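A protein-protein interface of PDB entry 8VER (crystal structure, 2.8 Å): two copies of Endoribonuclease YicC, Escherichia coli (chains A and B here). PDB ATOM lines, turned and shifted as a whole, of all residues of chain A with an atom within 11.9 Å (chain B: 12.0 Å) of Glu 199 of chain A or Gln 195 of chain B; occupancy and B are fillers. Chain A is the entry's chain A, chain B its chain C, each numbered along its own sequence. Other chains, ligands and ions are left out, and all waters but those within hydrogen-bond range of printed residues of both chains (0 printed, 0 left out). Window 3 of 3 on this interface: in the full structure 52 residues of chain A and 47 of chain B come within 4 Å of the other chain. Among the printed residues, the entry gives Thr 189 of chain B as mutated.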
ATOM      1  N   LEU A 187      -0.349  -2.576 -17.968  1.00  0.00           N
ATOM      2  CA  LEU A 187       1.017  -3.084 -18.039  1.00  0.00           C
ATOM      3  C   LEU A 187       1.151  -4.192 -19.076  1.00  0.00           C
ATOM      4  O   LEU A 187       2.163  -4.264 -19.785  1.00  0.00           O
ATOM      5  CB  LEU A 187       1.467  -3.578 -16.665  1.00  0.00           C
ATOM      6  CG  LEU A 187       1.543  -2.517 -15.566  1.00  0.00           C
ATOM      7  CD1 LEU A 187       2.184  -3.086 -14.310  1.00  0.00           C
ATOM      8  CD2 LEU A 187       2.296  -1.287 -16.049  1.00  0.00           C
ATOM      9  N   VAL A 188       0.150  -5.070 -19.180  1.00  0.00           N
ATOM     10  CA  VAL A 188       0.234  -6.143 -20.165  1.00  0.00           C
ATOM     11  C   VAL A 188       0.130  -5.584 -21.578  1.00  0.00           C
ATOM     12  O   VAL A 188       0.677  -6.166 -22.522  1.00  0.00           O
ATOM     13  CB  VAL A 188      -0.841  -7.217 -19.901  1.00  0.00           C
ATOM     14  CG1 VAL A 188      -0.681  -7.797 -18.504  1.00  0.00           C
ATOM     15  CG2 VAL A 188      -2.241  -6.650 -20.098  1.00  0.00           C
ATOM     16  N   LEU A 191       3.575  -4.454 -22.671  1.00  0.00           N
ATOM     17  CA  LEU A 191       4.416  -5.595 -23.018  1.00  0.00           C
ATOM     18  C   LEU A 191       4.098  -6.109 -24.417  1.00  0.00           C
ATOM     19  O   LEU A 191       5.003  -6.511 -25.157  1.00  0.00           O
ATOM     20  CB  LEU A 191       4.249  -6.707 -21.984  1.00  0.00           C
ATOM     21  CG  LEU A 191       5.341  -6.837 -20.919  1.00  0.00           C
ATOM     22  CD1 LEU A 191       5.542  -5.526 -20.177  1.00  0.00           C
ATOM     23  CD2 LEU A 191       5.003  -7.956 -19.948  1.00  0.00           C
ATOM     24  N   GLU A 192       2.818  -6.105 -24.798  1.00  0.00           N
ATOM     25  CA  GLU A 192       2.453  -6.533 -26.144  1.00  0.00           C
ATOM     26  C   GLU A 192       2.954  -5.554 -27.198  1.00  0.00           C
ATOM     27  O   GLU A 192       3.225  -5.956 -28.335  1.00  0.00           O
ATOM     28  CB  GLU A 192       0.937  -6.699 -26.256  1.00  0.00           C
ATOM     29  CG  GLU A 192       0.332  -7.645 -25.232  1.00  0.00           C
ATOM     30  CD  GLU A 192       0.903  -9.046 -25.313  1.00  0.00           C
ATOM     31  OE1 GLU A 192       1.144  -9.529 -26.438  1.00  0.00           O
ATOM     32  OE2 GLU A 192       1.114  -9.662 -24.247  1.00  0.00           O
ATOM     33  N   GLN A 195       6.263  -6.563 -27.831  1.00  0.00           N
ATOM     34  CA  GLN A 195       6.266  -7.997 -28.134  1.00  0.00           C
ATOM     35  C   GLN A 195       7.111  -8.783 -27.134  1.00  0.00           C
ATOM     36  O   GLN A 195       7.822  -9.721 -27.497  1.00  0.00           O
ATOM     37  CB  GLN A 195       6.731  -8.265 -29.568  1.00  0.00           C
ATOM     38  CG  GLN A 195       5.707  -7.908 -30.636  1.00  0.00           C
ATOM     39  CD  GLN A 195       5.714  -6.434 -30.987  1.00  0.00           C
ATOM     40  OE1 GLN A 195       6.761  -5.787 -30.977  1.00  0.00           O
ATOM     41  NE2 GLN A 195       4.542  -5.896 -31.301  1.00  0.00           N
ATOM     42  N   VAL A 196       7.031  -8.397 -25.861  1.00  0.00           N
ATOM     43  CA  VAL A 196       7.729  -9.129 -24.812  1.00  0.00           C
ATOM     44  C   VAL A 196       6.987 -10.428 -24.532  1.00  0.00           C
ATOM     45  O   VAL A 196       5.762 -10.435 -24.350  1.00  0.00           O
ATOM     46  CB  VAL A 196       7.855  -8.273 -23.544  1.00  0.00           C
ATOM     47  CG1 VAL A 196       8.533  -9.063 -22.434  1.00  0.00           C
ATOM     48  CG2 VAL A 196       8.629  -6.998 -23.839  1.00  0.00           C
ATOM     49  N   GLN A 197       7.725 -11.535 -24.504  1.00  0.00           N
ATOM     50  CA  GLN A 197       7.112 -12.835 -24.273  1.00  0.00           C
ATOM     51  C   GLN A 197       6.534 -12.912 -22.866  1.00  0.00           C
ATOM     52  O   GLN A 197       7.173 -12.510 -21.889  1.00  0.00           O
ATOM     53  CB  GLN A 197       8.137 -13.951 -24.477  1.00  0.00           C
ATOM     54  CG  GLN A 197       8.925 -13.847 -25.771  1.00  0.00           C
ATOM     55  CD  GLN A 197       8.063 -14.027 -27.003  1.00  0.00           C
ATOM     56  OE1 GLN A 197       7.125 -14.826 -27.011  1.00  0.00           O
ATOM     57  NE2 GLN A 197       8.376 -13.282 -28.053  1.00  0.00           N
ATOM     58  N   LEU A 198       5.314 -13.432 -22.768  1.00  0.00           N
ATOM     59  CA  LEU A 198       4.659 -13.584 -21.479  1.00  0.00           C
ATOM     60  C   LEU A 198       5.211 -14.791 -20.731  1.00  0.00           C
ATOM     61  O   LEU A 198       5.591 -15.802 -21.330  1.00  0.00           O
ATOM     62  CB  LEU A 198       3.149 -13.736 -21.657  1.00  0.00           C
ATOM     63  CG  LEU A 198       2.395 -12.550 -22.259  1.00  0.00           C
ATOM     64  CD1 LEU A 198       0.917 -12.883 -22.383  1.00  0.00           C
ATOM     65  CD2 LEU A 198       2.601 -11.300 -21.417  1.00  0.00           C
ATOM     66  N   GLU A 199       5.256 -14.673 -19.407  1.00  0.00           N
ATOM     67  CA  GLU A 199       5.655 -15.768 -18.536  1.00  0.00           C
ATOM     68  C   GLU A 199       4.465 -16.603 -18.078  1.00  0.00           C
ATOM     69  O   GLU A 199       4.631 -17.495 -17.241  1.00  0.00           O
ATOM     70  CB  GLU A 199       6.415 -15.221 -17.323  1.00  0.00           C
ATOM     71  CG  GLU A 199       7.430 -16.184 -16.727  1.00  0.00           C
ATOM     72  CD  GLU A 199       8.613 -16.426 -17.643  1.00  0.00           C
ATOM     73  OE1 GLU A 199       8.920 -15.540 -18.469  1.00  0.00           O
ATOM     74  OE2 GLU A 199       9.233 -17.504 -17.537  1.00  0.00           O
ATOM     75  N   ASN A 200       3.272 -16.323 -18.609  1.00  0.00           N
ATOM     76  CA  ASN A 200       2.044 -17.067 -18.312  1.00  0.00           C
ATOM     77  C   ASN A 200       1.740 -16.930 -16.825  1.00  0.00           C
ATOM     78  O   ASN A 200       1.553 -15.792 -16.359  1.00  0.00           O
ATOM     79  CB  ASN A 200       2.186 -18.499 -18.834  1.00  0.00           C
ATOM     80  CG  ASN A 200       2.069 -18.582 -20.341  1.00  0.00           C
ATOM     81  OD1 ASN A 200       1.532 -17.681 -20.985  1.00  0.00           O
ATOM     82  ND2 ASN A 200       2.564 -19.674 -20.913  1.00  0.00           N
ATOM     83  N   ASN A 201       1.685 -18.018 -16.053  1.00  0.00           N
ATOM     84  CA  ASN A 201       1.210 -17.931 -14.675  1.00  0.00           C
ATOM     85  C   ASN A 201       2.170 -17.143 -13.793  1.00  0.00           C
ATOM     86  O   ASN A 201       1.733 -16.409 -12.899  1.00  0.00           O
ATOM     87  CB  ASN A 201       0.987 -19.332 -14.108  1.00  0.00           C
ATOM     88  CG  ASN A 201      -0.201 -20.028 -14.739  1.00  0.00           C
ATOM     89  OD1 ASN A 201      -0.836 -19.489 -15.645  1.00  0.00           O
ATOM     90  ND2 ASN A 201      -0.504 -21.234 -14.270  1.00  0.00           N
ATOM     91  N   ARG A 202       3.478 -17.279 -14.022  1.00  0.00           N
ATOM     92  CA  ARG A 202       4.436 -16.561 -13.189  1.00  0.00           C
ATOM     93  C   ARG A 202       4.322 -15.052 -13.385  1.00  0.00           C
ATOM     94  O   ARG A 202       4.502 -14.284 -12.432  1.00  0.00           O
ATOM     95  CB  ARG A 202       5.858 -17.039 -13.480  1.00  0.00           C
ATOM     96  CG  ARG A 202       6.884 -16.494 -12.503  1.00  0.00           C
ATOM     97  CD  ARG A 202       8.208 -17.226 -12.603  1.00  0.00           C
ATOM     98  NE  ARG A 202       9.009 -17.027 -11.402  1.00  0.00           N
ATOM     99  CZ  ARG A 202       9.860 -16.026 -11.225  1.00  0.00           C
ATOM    100  NH1 ARG A 202      10.063 -15.117 -12.164  1.00  0.00           N
ATOM    101  NH2 ARG A 202      10.526 -15.937 -10.078  1.00  0.00           N
ATOM    102  N   LEU A 203       4.024 -14.609 -14.610  1.00  0.00           N
ATOM    103  CA  LEU A 203       3.769 -13.189 -14.842  1.00  0.00           C
ATOM    104  C   LEU A 203       2.553 -12.724 -14.051  1.00  0.00           C
ATOM    105  O   LEU A 203       2.573 -11.658 -13.425  1.00  0.00           O
ATOM    106  CB  LEU A 203       3.577 -12.924 -16.339  1.00  0.00           C
ATOM    107  CG  LEU A 203       3.517 -11.489 -16.897  1.00  0.00           C
ATOM    108  CD1 LEU A 203       2.135 -10.844 -16.756  1.00  0.00           C
ATOM    109  CD2 LEU A 203       4.587 -10.604 -16.269  1.00  0.00           C
ATOM    110  N   GLU A 204       1.481 -13.517 -14.071  1.00  0.00           N
ATOM    111  CA  GLU A 204       0.264 -13.134 -13.364  1.00  0.00           C
ATOM    112  C   GLU A 204       0.501 -13.062 -11.861  1.00  0.00           C
ATOM    113  O   GLU A 204      -0.077 -12.213 -11.173  1.00  0.00           O
ATOM    114  CB  GLU A 204      -0.855 -14.120 -13.691  1.00  0.00           C
ATOM    115  CG  GLU A 204      -1.071 -14.331 -15.179  1.00  0.00           C
ATOM    116  CD  GLU A 204      -1.735 -15.657 -15.482  1.00  0.00           C
ATOM    117  OE1 GLU A 204      -2.162 -16.338 -14.527  1.00  0.00           O
ATOM    118  OE2 GLU A 204      -1.824 -16.022 -16.674  1.00  0.00           O
ATOM    119  N   GLN A 205       1.356 -13.942 -11.333  1.00  0.00           N
ATOM    120  CA  GLN A 205       1.661 -13.916  -9.906  1.00  0.00           C
ATOM    121  C   GLN A 205       2.440 -12.662  -9.531  1.00  0.00           C
ATOM    122  O   GLN A 205       2.117 -11.992  -8.545  1.00  0.00           O
ATOM    123  CB  GLN A 205       2.438 -15.171  -9.511  1.00  0.00           C
ATOM    124  CG  GLN A 205       1.694 -16.468  -9.768  1.00  0.00           C
ATOM    125  CD  GLN A 205       0.387 -16.549  -9.008  1.00  0.00           C
ATOM    126  OE1 GLN A 205      -0.600 -17.092  -9.504  1.00  0.00           O
ATOM    127  NE2 GLN A 205       0.378 -16.025  -7.786  1.00  0.00           N
ATOM    128  N   GLU A 206       3.474 -12.329 -10.305  1.00  0.00           N
ATOM    129  CA  GLU A 206       4.253 -11.133 -10.004  1.00  0.00           C
ATOM    130  C   GLU A 206       3.434  -9.864 -10.206  1.00  0.00           C
ATOM    131  O   GLU A 206       3.700  -8.846  -9.556  1.00  0.00           O
ATOM    132  CB  GLU A 206       5.513 -11.099 -10.867  1.00  0.00           C
ATOM    133  CG  GLU A 206       6.512 -12.197 -10.541  1.00  0.00           C
ATOM    134  CD  GLU A 206       7.530 -12.400 -11.644  1.00  0.00           C
ATOM    135  OE1 GLU A 206       7.146 -12.294 -12.827  1.00  0.00           O
ATOM    136  OE2 GLU A 206       8.711 -12.656 -11.329  1.00  0.00           O
ATOM    137  N   LEU A 207       2.432  -9.907 -11.086  1.00  0.00           N
ATOM    138  CA  LEU A 207       1.628  -8.719 -11.349  1.00  0.00           C
ATOM    139  C   LEU A 207       0.775  -8.352 -10.142  1.00  0.00           C
ATOM    140  O   LEU A 207       0.650  -7.170  -9.800  1.00  0.00           O
ATOM    141  CB  LEU A 207       0.752  -8.943 -12.581  1.00  0.00           C
ATOM    142  CG  LEU A 207      -0.110  -7.766 -13.038  1.00  0.00           C
ATOM    143  CD1 LEU A 207       0.754  -6.567 -13.398  1.00  0.00           C
ATOM    144  CD2 LEU A 207      -0.983  -8.171 -14.214  1.00  0.00           C
ATOM    145  N   VAL A 208       0.185  -9.347  -9.480  1.00  0.00           N
ATOM    146  CA  VAL A 208      -0.658  -9.052  -8.327  1.00  0.00           C
ATOM    147  C   VAL A 208       0.186  -8.791  -7.083  1.00  0.00           C
ATOM    148  O   VAL A 208      -0.254  -8.079  -6.173  1.00  0.00           O
ATOM    149  CB  VAL A 208      -1.673 -10.185  -8.095  1.00  0.00           C
ATOM    150  CG1 VAL A 208      -2.572 -10.346  -9.313  1.00  0.00           C
ATOM    151  CG2 VAL A 208      -0.961 -11.487  -7.782  1.00  0.00           C
ATOM    152  N   LEU B 187      12.632  -2.084 -22.923  1.00  0.00           N
ATOM    153  CA  LEU B 187      12.126  -3.387 -22.502  1.00  0.00           C
ATOM    154  C   LEU B 187      12.910  -4.522 -23.150  1.00  0.00           C
ATOM    155  O   LEU B 187      13.292  -5.487 -22.477  1.00  0.00           O
ATOM    156  CB  LEU B 187      10.638  -3.500 -22.833  1.00  0.00           C
ATOM    157  CG  LEU B 187       9.703  -2.650 -21.971  1.00  0.00           C
ATOM    158  CD1 LEU B 187       8.311  -2.607 -22.572  1.00  0.00           C
ATOM    159  CD2 LEU B 187       9.654  -3.190 -20.551  1.00  0.00           C
ATOM    160  N   VAL B 188      13.156  -4.430 -24.459  1.00  0.00           N
ATOM    161  CA  VAL B 188      13.882  -5.493 -25.146  1.00  0.00           C
ATOM    162  C   VAL B 188      15.341  -5.524 -24.709  1.00  0.00           C
ATOM    163  O   VAL B 188      15.992  -6.574 -24.768  1.00  0.00           O
ATOM    164  CB  VAL B 188      13.754  -5.332 -26.673  1.00  0.00           C
ATOM    165  CG1 VAL B 188      12.290  -5.310 -27.080  1.00  0.00           C
ATOM    166  CG2 VAL B 188      14.456  -4.068 -27.146  1.00  0.00           C
ATOM    167  N   THR B 189      15.879  -4.385 -24.265  1.00  0.00           N
ATOM    168  CA  THR B 189      17.261  -4.361 -23.802  1.00  0.00           C
ATOM    169  C   THR B 189      17.408  -5.071 -22.463  1.00  0.00           C
ATOM    170  O   THR B 189      18.428  -5.726 -22.216  1.00  0.00           O
ATOM    171  CB  THR B 189      17.762  -2.917 -23.702  1.00  0.00           C
ATOM    172  OG1 THR B 189      17.534  -2.244 -24.946  1.00  0.00           O
ATOM    173  CG2 THR B 189      19.252  -2.886 -23.393  1.00  0.00           C
ATOM    174  N   LYS B 190      16.401  -4.965 -21.594  1.00  0.00           N
ATOM    175  CA  LYS B 190      16.436  -5.691 -20.331  1.00  0.00           C
ATOM    176  C   LYS B 190      16.359  -7.199 -20.533  1.00  0.00           C
ATOM    177  O   LYS B 190      16.810  -7.951 -19.662  1.00  0.00           O
ATOM    178  CB  LYS B 190      15.298  -5.223 -19.425  1.00  0.00           C
ATOM    179  CG  LYS B 190      15.377  -3.753 -19.041  1.00  0.00           C
ATOM    180  CD  LYS B 190      16.654  -3.435 -18.277  1.00  0.00           C
ATOM    181  CE  LYS B 190      16.704  -1.965 -17.892  1.00  0.00           C
ATOM    182  NZ  LYS B 190      17.935  -1.623 -17.128  1.00  0.00           N
ATOM    183  N   LEU B 191      15.802  -7.655 -21.655  1.00  0.00           N
ATOM    184  CA  LEU B 191      15.767  -9.080 -21.983  1.00  0.00           C
ATOM    185  C   LEU B 191      17.126  -9.500 -22.544  1.00  0.00           C
ATOM    186  O   LEU B 191      17.305  -9.743 -23.739  1.00  0.00           O
ATOM    187  CB  LEU B 191      14.643  -9.380 -22.964  1.00  0.00           C
ATOM    188  CG  LEU B 191      13.266  -9.675 -22.369  1.00  0.00           C
ATOM    189  CD1 LEU B 191      12.234  -9.797 -23.476  1.00  0.00           C
ATOM    190  CD2 LEU B 191      13.308 -10.943 -21.533  1.00  0.00           C
ATOM    191  N   GLU B 192      18.101  -9.578 -21.644  1.00  0.00           N
ATOM    192  CA  GLU B 192      19.447 -10.017 -21.978  1.00  0.00           C
ATOM    193  C   GLU B 192      19.707 -11.379 -21.350  1.00  0.00           C
ATOM    194  O   GLU B 192      19.326 -11.625 -20.201  1.00  0.00           O
ATOM    195  CB  GLU B 192      20.491  -9.003 -21.504  1.00  0.00           C
ATOM    196  CG  GLU B 192      20.392  -8.638 -20.036  1.00  0.00           C
ATOM    197  CD  GLU B 192      21.431  -7.617 -19.628  1.00  0.00           C
ATOM    198  OE1 GLU B 192      22.271  -7.253 -20.478  1.00  0.00           O
ATOM    199  OE2 GLU B 192      21.408  -7.176 -18.460  1.00  0.00           O
ATOM    200  N   ASP B 193      20.353 -12.261 -22.117  1.00  0.00           N
ATOM    201  CA  ASP B 193      20.604 -13.642 -21.700  1.00  0.00           C
ATOM    202  C   ASP B 193      19.297 -14.342 -21.335  1.00  0.00           C
ATOM    203  O   ASP B 193      19.169 -14.968 -20.280  1.00  0.00           O
ATOM    204  CB  ASP B 193      21.599 -13.698 -20.537  1.00  0.00           C
ATOM    205  CG  ASP B 193      22.898 -12.990 -20.852  1.00  0.00           C
ATOM    206  OD1 ASP B 193      23.359 -13.087 -22.008  1.00  0.00           O
ATOM    207  OD2 ASP B 193      23.454 -12.333 -19.946  1.00  0.00           O
ATOM    208  N   ALA B 194      18.314 -14.226 -22.224  1.00  0.00           N
ATOM    209  CA  ALA B 194      16.995 -14.774 -21.951  1.00  0.00           C
ATOM    210  C   ALA B 194      17.011 -16.293 -22.058  1.00  0.00           C
ATOM    211  O   ALA B 194      17.670 -16.865 -22.932  1.00  0.00           O
ATOM    212  CB  ALA B 194      15.964 -14.183 -22.915  1.00  0.00           C
ATOM    213  N   GLN B 195      16.288 -16.944 -21.153  1.00  0.00           N
ATOM    214  CA  GLN B 195      16.211 -18.398 -21.112  1.00  0.00           C
ATOM    215  C   GLN B 195      15.620 -18.960 -22.400  1.00  0.00           C
ATOM    216  O   GLN B 195      16.270 -19.730 -23.106  1.00  0.00           O
ATOM    217  CB  GLN B 195      15.378 -18.851 -19.912  1.00  0.00           C
ATOM    218  CG  GLN B 195      13.986 -18.240 -19.872  1.00  0.00           C
ATOM    219  CD  GLN B 195      13.244 -18.562 -18.590  1.00  0.00           C
ATOM    220  OE1 GLN B 195      13.644 -19.444 -17.831  1.00  0.00           O
ATOM    221  NE2 GLN B 195      12.157 -17.840 -18.340  1.00  0.00           N
ATOM    222  N   ASN B 201      20.144 -15.983 -15.065  1.00  0.00           N
ATOM    223  CA  ASN B 201      19.515 -17.241 -14.684  1.00  0.00           C
ATOM    224  C   ASN B 201      18.706 -17.089 -13.400  1.00  0.00           C
ATOM    225  O   ASN B 201      18.070 -18.038 -12.942  1.00  0.00           O
ATOM    226  CB  ASN B 201      20.569 -18.338 -14.515  1.00  0.00           C
ATOM    227  CG  ASN B 201      21.226 -18.721 -15.828  1.00  0.00           C
ATOM    228  OD1 ASN B 201      21.029 -18.061 -16.848  1.00  0.00           O
ATOM    229  ND2 ASN B 201      22.017 -19.788 -15.806  1.00  0.00           N
ATOM    230  N   ARG B 202      18.736 -15.890 -12.823  1.00  0.00           N
ATOM    231  CA  ARG B 202      17.971 -15.620 -11.613  1.00  0.00           C
ATOM    232  C   ARG B 202      16.488 -15.510 -11.946  1.00  0.00           C
ATOM    233  O   ARG B 202      16.104 -14.834 -12.906  1.00  0.00           O
ATOM    234  CB  ARG B 202      18.458 -14.335 -10.946  1.00  0.00           C
ATOM    235  CG  ARG B 202      19.918 -14.353 -10.529  1.00  0.00           C
ATOM    236  CD  ARG B 202      20.312 -13.032  -9.894  1.00  0.00           C
ATOM    237  NE  ARG B 202      21.736 -12.971  -9.593  1.00  0.00           N
ATOM    238  CZ  ARG B 202      22.348 -11.907  -9.091  1.00  0.00           C
ATOM    239  NH1 ARG B 202      21.686 -10.794  -8.819  1.00  0.00           N
ATOM    240  NH2 ARG B 202      23.656 -11.959  -8.858  1.00  0.00           N
ATOM    241  N   LEU B 203      15.653 -16.177 -11.150  1.00  0.00           N
ATOM    242  CA  LEU B 203      14.206 -16.161 -11.351  1.00  0.00           C
ATOM    243  C   LEU B 203      13.653 -14.866 -10.766  1.00  0.00           C
ATOM    244  O   LEU B 203      13.212 -14.811  -9.617  1.00  0.00           O
ATOM    245  CB  LEU B 203      13.558 -17.387 -10.718  1.00  0.00           C
ATOM    246  CG  LEU B 203      13.947 -18.741 -11.319  1.00  0.00           C
ATOM    247  CD1 LEU B 203      13.223 -19.878 -10.612  1.00  0.00           C
ATOM    248  CD2 LEU B 203      13.662 -18.771 -12.813  1.00  0.00           C
ATOM    249  N   GLU B 204      13.684 -13.809 -11.573  1.00  0.00           N
ATOM    250  CA  GLU B 204      13.166 -12.509 -11.169  1.00  0.00           C
ATOM    251  C   GLU B 204      12.846 -11.717 -12.428  1.00  0.00           C
ATOM    252  O   GLU B 204      13.636 -11.706 -13.375  1.00  0.00           O
ATOM    253  CB  GLU B 204      14.174 -11.755 -10.291  1.00  0.00           C
ATOM    254  CG  GLU B 204      13.594 -10.566  -9.535  1.00  0.00           C
ATOM    255  CD  GLU B 204      13.647  -9.273 -10.329  1.00  0.00           C
ATOM    256  OE1 GLU B 204      14.297  -9.249 -11.396  1.00  0.00           O
ATOM    257  OE2 GLU B 204      13.040  -8.278  -9.882  1.00  0.00           O
ATOM    258  N   GLN B 205      11.685 -11.065 -12.436  1.00  0.00           N
ATOM    259  CA  GLN B 205      11.209 -10.327 -13.605  1.00  0.00           C
ATOM    260  C   GLN B 205      11.018  -8.861 -13.228  1.00  0.00           C
ATOM    261  O   GLN B 205      10.031  -8.498 -12.579  1.00  0.00           O
ATOM    262  CB  GLN B 205       9.920 -10.937 -14.153  1.00  0.00           C
ATOM    263  CG  GLN B 205      10.067 -12.380 -14.620  1.00  0.00           C
ATOM    264  CD  GLN B 205      11.206 -12.568 -15.609  1.00  0.00           C
ATOM    265  OE1 GLN B 205      11.497 -11.685 -16.418  1.00  0.00           O
ATOM    266  NE2 GLN B 205      11.858 -13.723 -15.545  1.00  0.00           N
ATOM    267  N   GLU B 206      11.967  -8.028 -13.639  1.00  0.00           N
ATOM    268  CA  GLU B 206      11.867  -6.584 -13.497  1.00  0.00           C
ATOM    269  C   GLU B 206      11.099  -5.937 -14.642  1.00  0.00           C
ATOM    270  O   GLU B 206      10.912  -4.717 -14.633  1.00  0.00           O
ATOM    271  CB  GLU B 206      13.265  -5.966 -13.408  1.00  0.00           C
ATOM    272  CG  GLU B 206      14.126  -6.232 -14.635  1.00  0.00           C
ATOM    273  CD  GLU B 206      15.459  -5.512 -14.585  1.00  0.00           C
ATOM    274  OE1 GLU B 206      15.704  -4.784 -13.601  1.00  0.00           O
ATOM    275  OE2 GLU B 206      16.260  -5.671 -15.530  1.00  0.00           O
ATOM    276  N   LEU B 207      10.658  -6.726 -15.626  1.00  0.00           N
ATOM    277  CA  LEU B 207       9.963  -6.164 -16.778  1.00  0.00           C
ATOM    278  C   LEU B 207       8.601  -5.606 -16.387  1.00  0.00           C
ATOM    279  O   LEU B 207       8.197  -4.543 -16.872  1.00  0.00           O
ATOM    280  CB  LEU B 207       9.815  -7.226 -17.866  1.00  0.00           C
ATOM    281  CG  LEU B 207      11.116  -7.767 -18.458  1.00  0.00           C
ATOM    282  CD1 LEU B 207      10.904  -9.165 -19.009  1.00  0.00           C
ATOM    283  CD2 LEU B 207      11.635  -6.836 -19.544  1.00  0.00           C
ATOM    284  N   VAL B 208       7.878  -6.312 -15.516  1.00  0.00           N
ATOM    285  CA  VAL B 208       6.593  -5.810 -15.043  1.00  0.00           C
ATOM    286  C   VAL B 208       6.783  -4.519 -14.252  1.00  0.00           C
ATOM    287  O   VAL B 208       5.968  -3.593 -14.348  1.00  0.00           O
ATOM    288  CB  VAL B 208       5.871  -6.895 -14.221  1.00  0.00           C
ATOM    289  CG1 VAL B 208       6.794  -7.469 -13.155  1.00  0.00           C
ATOM    290  CG2 VAL B 208       4.598  -6.343 -13.596  1.00  0.00           C
ATOM    291  N   LEU B 209       7.866  -4.427 -13.474  1.00  0.00           N
ATOM    292  CA  LEU B 209       8.163  -3.189 -12.760  1.00  0.00           C
ATOM    293  C   LEU B 209       8.520  -2.069 -13.728  1.00  0.00           C
ATOM    294  O   LEU B 209       8.072  -0.929 -13.559  1.00  0.00           O
ATOM    295  CB  LEU B 209       9.300  -3.417 -11.758  1.00  0.00           C
ATOM    296  CG  LEU B 209       9.671  -2.344 -10.720  1.00  0.00           C
ATOM    297  CD1 LEU B 209      10.604  -1.272 -11.282  1.00  0.00           C
ATOM    298  CD2 LEU B 209       8.426  -1.706 -10.112  1.00  0.00           C
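O of Leu 191 of chain A sits at hydrogen-bond distance from N of Val 196 of chain A, 2.9 Å away. OE2 of Glu 206 of chain A is in salt-bridge range of NH1 of Arg 202 of chain A (2.9 Å). N of Glu 206 of chain B is in hydrogen-bond range of OE1 of Glu 204 of chain B, at 3.5 Å.
Hydrophobic or aromatic side chains of chain B that line the printed part of chain A: Leu 191, Leu 203 and Val 208. Along chain B the printed residues that touch a printed residue of chain A span positions 191 to 208. Hydrophobic or aromatic side chains of chain A that line the printed part of chain B: Leu 187, Val 196 and Leu 207. Among the printed residues, 8 pairs touch across the chains. Among the printed residues, no Asp or Glu carboxylate lies within 4 Å of a Lys or Arg side-chain nitrogen of the other chain.
The side-chain amide nitrogen (NE2) of Gln 195 of chain B is in hydrogen-bond range of the side-chain carboxylate (OE2) of Glu 199 of chain A, at 3.1 Å. NH2 of Arg 202 of chain A sits at hydrogen-bond distance from O of Leu 203 of chain B (2.9 Å).
Of chain B, only Gln 195 (3.1 Å) comes within 4 Å of Glu 199 of chain A. Of chain A, only Glu 199 comes within 4 Å of Gln 195 of chain B. No residue of chain B comes within 4 Å of Asn 200 of chain A. No residue of chain B comes within 4 Å of Asn 201 of chain A. Printed residues of chain A within 4 Å of Gln 205 of chain B: Arg 202 (3.7 Å) and Glu 206 (3.4 Å). Printed residues of chain B within 4 Å of Val 196 of chain A: Leu 191 (3.9 Å). Printed residues of chain A within 4 Å of Leu 203 of chain B: Arg 202. The nearest residue of chain A that does not touch Gln 195 of chain B is Arg 202 of chain A (7.0 Å). The nearest printed residue of chain A that does not touch Glu 204 of chain B is Glu 206 of chain A (4.4 Å).
Leu 187 of chain A touches Val 208 of chain B (CD1 to O, 3.8 Å). Leu 191 of chain B touches Val 196 of chain A. NH1 of Arg 202 of chain A touches N of Glu 204 of chain B (3.9 Å). Arg 202 of chain A touches Gln 205 of chain B. Glu 206 of chain A touches Gln 205 of chain B (OE1 to CB, 3.4 Å). Leu 207 of chain A touches Val 208 of chain B.
Arg 202 of chain A touches Leu 203 of chain B, but with the chains exchanged Leu 203 of chain A does not touch Arg 202 of chain B (12.2 Å). Arg 202 of chain A touches Gln 205 of chain B, but with the chains exchanged Gln 205 of chain A does not touch Arg 202 of chain B (14.1 Å). Glu 206 of chain A touches Gln 205 of chain B, but with the chains exchanged Gln 205 of chain A does not touch Glu 206 of chain B (11.4 Å). Leu 207 of chain A touches Val 208 of chain B, but with the chains exchanged Val 208 of chain A does not touch Leu 207 of chain B (11.5 Å). Of the 8 pairs that touch across the chains among the printed residues, none has its exchanged pair printed and touching as well.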
